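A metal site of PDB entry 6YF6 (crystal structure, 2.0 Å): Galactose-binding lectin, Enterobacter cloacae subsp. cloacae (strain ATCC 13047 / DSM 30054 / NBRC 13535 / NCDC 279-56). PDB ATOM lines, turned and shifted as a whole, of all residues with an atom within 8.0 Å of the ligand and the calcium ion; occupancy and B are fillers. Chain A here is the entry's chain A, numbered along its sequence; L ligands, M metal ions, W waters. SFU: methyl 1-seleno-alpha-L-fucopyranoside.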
ATOM      1  N   PHE A  40     -13.167  32.305  10.680  1.00  0.00           N
ATOM      2  CA  PHE A  40     -13.544  32.812  12.002  1.00  0.00           C
ATOM      3  C   PHE A  40     -13.444  31.647  12.977  1.00  0.00           C
ATOM      4  O   PHE A  40     -14.370  30.841  13.096  1.00  0.00           O
ATOM      5  CB  PHE A  40     -14.943  33.410  11.985  1.00  0.00           C
ATOM      6  CG  PHE A  40     -15.106  34.560  11.025  1.00  0.00           C
ATOM      7  CD1 PHE A  40     -15.259  34.344   9.670  1.00  0.00           C
ATOM      8  CD2 PHE A  40     -15.113  35.868  11.487  1.00  0.00           C
ATOM      9  CE1 PHE A  40     -15.410  35.395   8.785  1.00  0.00           C
ATOM     10  CE2 PHE A  40     -15.262  36.934  10.618  1.00  0.00           C
ATOM     11  CZ  PHE A  40     -15.411  36.703   9.260  1.00  0.00           C
ATOM     12  N   ILE A  41     -12.305  31.551  13.674  1.00  0.00           N
ATOM     13  CA  ILE A  41     -12.077  30.485  14.646  1.00  0.00           C
ATOM     14  C   ILE A  41     -12.496  30.873  16.061  1.00  0.00           C
ATOM     15  O   ILE A  41     -12.547  30.004  16.944  1.00  0.00           O
ATOM     16  CB  ILE A  41     -10.596  30.073  14.594  1.00  0.00           C
ATOM     17  CG1 ILE A  41     -10.408  28.643  15.123  1.00  0.00           C
ATOM     18  CG2 ILE A  41      -9.752  31.061  15.360  1.00  0.00           C
ATOM     19  CD1 ILE A  41     -11.045  27.573  14.244  1.00  0.00           C
ATOM     20  N   THR A  42     -12.792  32.153  16.304  1.00  0.00           N
ATOM     21  CA  THR A  42     -13.291  32.666  17.578  1.00  0.00           C
ATOM     22  C   THR A  42     -12.563  32.071  18.787  1.00  0.00           C
ATOM     23  O   THR A  42     -13.048  31.122  19.409  1.00  0.00           O
ATOM     24  CB  THR A  42     -14.797  32.437  17.693  1.00  0.00           C
ATOM     25  OG1 THR A  42     -15.104  31.043  17.555  1.00  0.00           O
ATOM     26  CG2 THR A  42     -15.515  33.205  16.603  1.00  0.00           C
ATOM     27  N   ARG A  43     -11.411  32.653  19.118  1.00  0.00           N
ATOM     28  CA  ARG A  43     -10.556  32.110  20.146  1.00  0.00           C
ATOM     29  C   ARG A  43     -11.174  32.289  21.529  1.00  0.00           C
ATOM     30  O   ARG A  43     -12.082  33.098  21.720  1.00  0.00           O
ATOM     31  CB  ARG A  43      -9.191  32.812  20.120  1.00  0.00           C
ATOM     32  CG  ARG A  43      -8.396  32.651  18.829  1.00  0.00           C
ATOM     33  CD  ARG A  43      -7.098  33.416  18.963  1.00  0.00           C
ATOM     34  NE  ARG A  43      -6.320  33.518  17.739  1.00  0.00           N
ATOM     35  CZ  ARG A  43      -5.141  34.134  17.668  1.00  0.00           C
ATOM     36  NH1 ARG A  43      -4.622  34.689  18.762  1.00  0.00           N
ATOM     37  NH2 ARG A  43      -4.477  34.198  16.525  1.00  0.00           N
ATOM     38  N   PRO A  44     -10.675  31.544  22.535  1.00  0.00           N
ATOM     39  CA  PRO A  44     -11.264  31.631  23.874  1.00  0.00           C
ATOM     40  C   PRO A  44     -11.182  33.027  24.471  1.00  0.00           C
ATOM     41  O   PRO A  44     -10.237  33.778  24.236  1.00  0.00           O
ATOM     42  CB  PRO A  44     -10.409  30.637  24.687  1.00  0.00           C
ATOM     43  CG  PRO A  44      -9.841  29.694  23.674  1.00  0.00           C
ATOM     44  CD  PRO A  44      -9.626  30.509  22.440  1.00  0.00           C
ATOM     45  N   ASN A  45     -12.221  33.367  25.239  1.00  0.00           N
ATOM     46  CA  ASN A  45     -12.213  34.533  26.121  1.00  0.00           C
ATOM     47  C   ASN A  45     -12.115  35.848  25.366  1.00  0.00           C
ATOM     48  O   ASN A  45     -11.494  36.806  25.838  1.00  0.00           O
ATOM     49  CB  ASN A  45     -11.089  34.440  27.153  1.00  0.00           C
ATOM     50  CG  ASN A  45     -11.272  33.268  28.098  1.00  0.00           C
ATOM     51  OD1 ASN A  45     -12.393  32.764  28.267  1.00  0.00           O
ATOM     52  ND2 ASN A  45     -10.190  32.834  28.721  1.00  0.00           N
ATOM     53  N   HIS A  48     -17.193  37.580  20.573  1.00  0.00           N
ATOM     54  CA  HIS A  48     -17.323  37.471  19.126  1.00  0.00           C
ATOM     55  C   HIS A  48     -18.703  37.887  18.616  1.00  0.00           C
ATOM     56  O   HIS A  48     -19.063  37.571  17.479  1.00  0.00           O
ATOM     57  CB  HIS A  48     -17.000  36.046  18.684  1.00  0.00           C
ATOM     58  CG  HIS A  48     -15.704  35.544  19.256  1.00  0.00           C
ATOM     59  ND1 HIS A  48     -14.482  35.944  18.765  1.00  0.00           N
ATOM     60  CD2 HIS A  48     -15.443  34.718  20.291  1.00  0.00           C
ATOM     61  CE1 HIS A  48     -13.518  35.375  19.463  1.00  0.00           C
ATOM     62  NE2 HIS A  48     -14.075  34.619  20.399  1.00  0.00           N
ATOM     63  N   ARG A  74     -20.607  27.148   8.116  1.00  0.00           N
ATOM     64  CA  ARG A  74     -20.073  26.683   9.378  1.00  0.00           C
ATOM     65  C   ARG A  74     -18.942  25.695   9.116  1.00  0.00           C
ATOM     66  O   ARG A  74     -18.923  24.993   8.108  1.00  0.00           O
ATOM     67  CB  ARG A  74     -21.160  26.018  10.219  1.00  0.00           C
ATOM     68  CG  ARG A  74     -20.704  25.710  11.645  1.00  0.00           C
ATOM     69  CD  ARG A  74     -21.711  24.864  12.376  1.00  0.00           C
ATOM     70  NE  ARG A  74     -21.464  24.868  13.811  1.00  0.00           N
ATOM     71  CZ  ARG A  74     -22.226  24.236  14.703  1.00  0.00           C
ATOM     72  NH1 ARG A  74     -23.290  23.540  14.302  1.00  0.00           N
ATOM     73  NH2 ARG A  74     -21.923  24.299  15.994  1.00  0.00           N
ATOM     74  N   ILE A  75     -17.985  25.658  10.039  1.00  0.00           N
ATOM     75  CA  ILE A  75     -16.941  24.643  10.011  1.00  0.00           C
ATOM     76  C   ILE A  75     -16.917  23.938  11.368  1.00  0.00           C
ATOM     77  O   ILE A  75     -17.419  24.441  12.372  1.00  0.00           O
ATOM     78  CB  ILE A  75     -15.553  25.223   9.678  1.00  0.00           C
ATOM     79  CG1 ILE A  75     -15.161  26.314  10.676  1.00  0.00           C
ATOM     80  CG2 ILE A  75     -15.556  25.759   8.250  1.00  0.00           C
ATOM     81  CD1 ILE A  75     -13.667  26.592  10.713  1.00  0.00           C
ATOM     82  N   ILE A  76     -16.326  22.739  11.370  1.00  0.00           N
ATOM     83  CA  ILE A  76     -16.145  21.939  12.576  1.00  0.00           C
ATOM     84  C   ILE A  76     -17.482  21.400  13.045  1.00  0.00           C
ATOM     85  O   ILE A  76     -17.663  20.182  13.188  1.00  0.00           O
ATOM     86  CB  ILE A  76     -15.439  22.753  13.679  1.00  0.00           C
ATOM     87  CG1 ILE A  76     -14.099  23.275  13.152  1.00  0.00           C
ATOM     88  CG2 ILE A  76     -15.249  21.907  14.917  1.00  0.00           C
ATOM     89  CD1 ILE A  76     -13.353  24.183  14.106  1.00  0.00           C
ATOM     90  N   GLY A  77     -18.442  22.297  13.300  1.00  0.00           N
ATOM     91  CA  GLY A  77     -19.784  21.875  13.644  1.00  0.00           C
ATOM     92  C   GLY A  77     -20.002  21.500  15.086  1.00  0.00           C
ATOM     93  O   GLY A  77     -20.997  20.828  15.401  1.00  0.00           O
ATOM     94  N   LYS A  78     -19.119  21.911  15.990  1.00  0.00           N
ATOM     95  CA  LYS A  78     -19.208  21.510  17.379  1.00  0.00           C
ATOM     96  C   LYS A  78     -19.546  22.707  18.259  1.00  0.00           C
ATOM     97  O   LYS A  78     -19.177  23.845  17.965  1.00  0.00           O
ATOM     98  CB  LYS A  78     -17.900  20.858  17.838  1.00  0.00           C
ATOM     99  CG  LYS A  78     -17.827  19.363  17.529  1.00  0.00           C
ATOM    100  CD  LYS A  78     -16.684  18.669  18.246  1.00  0.00           C
ATOM    101  CE  LYS A  78     -16.672  18.954  19.742  1.00  0.00           C
ATOM    102  NZ  LYS A  78     -16.503  17.742  20.575  1.00  0.00           N
ATOM    103  N   TYR A  79     -20.239  22.413  19.346  1.00  0.00           N
ATOM    104  CA  TYR A  79     -20.618  23.416  20.361  1.00  0.00           C
ATOM    105  C   TYR A  79     -21.554  24.425  19.679  1.00  0.00           C
ATOM    106  O   TYR A  79     -22.447  24.026  18.932  1.00  0.00           O
ATOM    107  CB  TYR A  79     -19.355  23.988  20.969  1.00  0.00           C
ATOM    108  CG  TYR A  79     -18.503  22.936  21.652  1.00  0.00           C
ATOM    109  CD1 TYR A  79     -17.131  22.890  21.466  1.00  0.00           C
ATOM    110  CD2 TYR A  79     -19.079  21.982  22.488  1.00  0.00           C
ATOM    111  CE1 TYR A  79     -16.355  21.921  22.090  1.00  0.00           C
ATOM    112  CE2 TYR A  79     -18.311  21.017  23.109  1.00  0.00           C
ATOM    113  CZ  TYR A  79     -16.950  20.989  22.914  1.00  0.00           C
ATOM    114  OH  TYR A  79     -16.190  20.029  23.531  1.00  0.00           O
ATOM    115  N   GLU A  80     -21.378  25.724  19.918  1.00  0.00           N
ATOM    116  CA  GLU A  80     -22.389  26.694  19.543  1.00  0.00           C
ATOM    117  C   GLU A  80     -22.392  26.953  18.040  1.00  0.00           C
ATOM    118  O   GLU A  80     -21.343  27.084  17.404  1.00  0.00           O
ATOM    119  CB  GLU A  80     -22.180  28.000  20.300  1.00  0.00           C
ATOM    120  CG  GLU A  80     -22.815  27.996  21.688  1.00  0.00           C
ATOM    121  CD  GLU A  80     -23.156  29.385  22.184  1.00  0.00           C
ATOM    122  OE1 GLU A  80     -22.607  29.795  23.221  1.00  0.00           O
ATOM    123  OE2 GLU A  80     -23.990  30.055  21.537  1.00  0.00           O
ATOM    124  N   ALA A 129     -19.893  33.533  21.955  1.00  0.00           N
ATOM    125  CA  ALA A 129     -19.157  32.410  22.501  1.00  0.00           C
ATOM    126  C   ALA A 129     -17.909  32.104  21.684  1.00  0.00           C
ATOM    127  O   ALA A 129     -17.828  32.388  20.482  1.00  0.00           O
ATOM    128  CB  ALA A 129     -20.048  31.165  22.539  1.00  0.00           C
ATOM    129  N   SER A 130     -16.922  31.510  22.352  1.00  0.00           N
ATOM    130  CA  SER A 130     -15.735  30.968  21.694  1.00  0.00           C
ATOM    131  C   SER A 130     -15.803  29.467  21.513  1.00  0.00           C
ATOM    132  O   SER A 130     -15.217  28.934  20.559  1.00  0.00           O
ATOM    133  CB  SER A 130     -14.476  31.325  22.496  1.00  0.00           C
ATOM    134  OG  SER A 130     -14.461  30.615  23.722  1.00  0.00           O
ATOM    135  N   MET A 131     -16.525  28.768  22.394  1.00  0.00           N
ATOM    136  CA  MET A 131     -16.755  27.335  22.253  1.00  0.00           C
ATOM    137  C   MET A 131     -17.592  27.084  21.009  1.00  0.00           C
ATOM    138  O   MET A 131     -18.799  27.373  20.999  1.00  0.00           O
ATOM    139  CB  MET A 131     -17.445  26.787  23.496  1.00  0.00           C
ATOM    140  CG  MET A 131     -16.565  26.714  24.735  1.00  0.00           C
ATOM    141  SD  MET A 131     -15.295  25.437  24.604  1.00  0.00           S
ATOM    142  CE  MET A 131     -16.282  23.946  24.722  1.00  0.00           C
ATOM    143  N   GLY A 132     -16.971  26.563  19.959  1.00  0.00           N
ATOM    144  CA  GLY A 132     -17.625  26.465  18.679  1.00  0.00           C
ATOM    145  C   GLY A 132     -17.693  27.825  18.004  1.00  0.00           C
ATOM    146  O   GLY A 132     -16.727  28.591  18.062  1.00  0.00           O
ATOM    147  N   ASN A 133     -18.816  28.137  17.377  1.00  0.00           N
ATOM    148  CA  ASN A 133     -18.989  29.422  16.712  1.00  0.00           C
ATOM    149  C   ASN A 133     -17.880  29.652  15.677  1.00  0.00           C
ATOM    150  O   ASN A 133     -17.278  30.722  15.609  1.00  0.00           O
ATOM    151  CB  ASN A 133     -19.023  30.557  17.741  1.00  0.00           C
ATOM    152  CG  ASN A 133     -19.529  31.851  17.161  1.00  0.00           C
ATOM    153  OD1 ASN A 133     -20.259  31.857  16.174  1.00  0.00           O
ATOM    154  ND2 ASN A 133     -19.145  32.964  17.766  1.00  0.00           N
ATOM    155  N   ASP A 134     -17.608  28.620  14.883  1.00  0.00           N
ATOM    156  CA  ASP A 134     -16.543  28.619  13.887  1.00  0.00           C
ATOM    157  C   ASP A 134     -17.142  28.575  12.487  1.00  0.00           C
ATOM    158  O   ASP A 134     -17.994  27.732  12.197  1.00  0.00           O
ATOM    159  CB  ASP A 134     -15.606  27.431  14.093  1.00  0.00           C
ATOM    160  CG  ASP A 134     -15.117  27.326  15.531  1.00  0.00           C
ATOM    161  OD1 ASP A 134     -14.464  28.275  16.002  1.00  0.00           O
ATOM    162  OD2 ASP A 134     -15.390  26.292  16.174  1.00  0.00           O
ATOM    163  N   PHE A 135     -16.683  29.457  11.601  1.00  0.00           N
ATOM    164  CA  PHE A 135     -17.269  29.559  10.277  1.00  0.00           C
ATOM    165  C   PHE A 135     -16.299  30.277   9.348  1.00  0.00           C
ATOM    166  O   PHE A 135     -15.276  30.822   9.767  1.00  0.00           O
ATOM    167  CB  PHE A 135     -18.625  30.279  10.317  1.00  0.00           C
ATOM    168  CG  PHE A 135     -18.588  31.627  10.991  1.00  0.00           C
ATOM    169  CD1 PHE A 135     -18.563  31.739  12.373  1.00  0.00           C
ATOM    170  CD2 PHE A 135     -18.596  32.790  10.231  1.00  0.00           C
ATOM    171  CE1 PHE A 135     -18.546  32.985  12.985  1.00  0.00           C
ATOM    172  CE2 PHE A 135     -18.568  34.028  10.838  1.00  0.00           C
ATOM    173  CZ  PHE A 135     -18.547  34.128  12.213  1.00  0.00           C
HETATM  174  C1  SFU L   1     -13.031  25.378  21.502  1.00  0.00           C
HETATM  175  C2  SFU L   1     -12.626  26.743  20.950  1.00  0.00           C
HETATM  176  C3  SFU L   1     -12.172  26.684  19.476  1.00  0.00           C
HETATM  177  C4  SFU L   1     -13.257  25.978  18.671  1.00  0.00           C
HETATM  178  C5  SFU L   1     -13.462  24.593  19.270  1.00  0.00           C
HETATM  179  C6  SFU L   1     -14.550  23.862  18.497  1.00  0.00           C
HETATM  180  O2  SFU L   1     -11.579  27.262  21.745  1.00  0.00           O
HETATM  181  O3  SFU L   1     -12.076  28.006  18.968  1.00  0.00           O
HETATM  182  O4  SFU L   1     -14.490  26.664  18.749  1.00  0.00           O
HETATM  183  O5  SFU L   1     -13.895  24.661  20.646  1.00  0.00           O
HETATM  184  CM  SFU L   1     -12.170  22.630  22.380  1.00  0.00           C
HETATM  185 SE   SFU L   1     -11.383  24.289  21.851  1.00  0.00          SE
HETATM  186 CA    CA M   1     -14.228  29.044  18.334  1.00  0.00          CA
HETATM  187  O   HOH W   1     -13.283  28.201  24.157  1.00  0.00           O
HETATM  188  O   HOH W   2      -9.529  28.960  18.941  1.00  0.00           O
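N of Gly 132 lies close to O4 of the ligand, at 2.8 Å.
The backbone carbonyl oxygen (O) of Asn 133 lies close to the side-chain hydroxyl (OG1) of Thr 42 (2.9 Å).
The backbone carbonyl oxygen (O) of Asp 134 is in hydrogen-bond range of the backbone NH (N) of Ile 75 (3.0 Å).
The guanidinium group (NH2) of Arg 74 lies within hydrogen-bond range of the backbone carbonyl oxygen (O) of Tyr 79, 3.0 Å away.
The backbone NH (N) of Glu 80 is in hydrogen-bond range of the backbone carbonyl oxygen (O) of Met 131, 3.2 Å away.
Residues that only touch the ligand: Pro 44 (3.6 Å), Tyr 79 (3.8 Å) and Met 131 (3.8 Å).
Hydrophobic or aromatic side chains within 4 Å of the ligand: Pro 44, Tyr 79 and Met 131.
Within 4 Å of the ligand: Ile 41, Thr 42, Pro 44, Tyr 79, Ser 130, Met 131, Gly 132 and Asp 134.
Along chain A the residues within 4 Å of the ligand span positions 41 to 134.
The nearest printed residue that does not touch the ligand is Ile 76 (4.1 Å).
Five residues have an atom within 4 Å of the calcium ion: Ile 41, Thr 42, Ser 130, Gly 132 and Asp 134.
The calcium ion is bound by OG1 of Thr 42 (2.3 Å), O of Ile 41 (2.4 Å), O4 of the ligand (2.4 Å), O of Ser 130 (2.4 Å), OD1 of Asp 134 (2.5 Å), O3 of the ligand (2.5 Å), O of Gly 132 (2.6 Å) and O of Thr 42 (2.6 Å).
The calcium ion has eight donor atoms within binding distance.
Water W1 lies within hydrogen-bond range of the side-chain hydroxyl of Ser 130 (2.7 Å), an oxygen (O2) of the ligand (3.1 Å) and the side-chain sulfur of Met 131 (3.4 Å).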
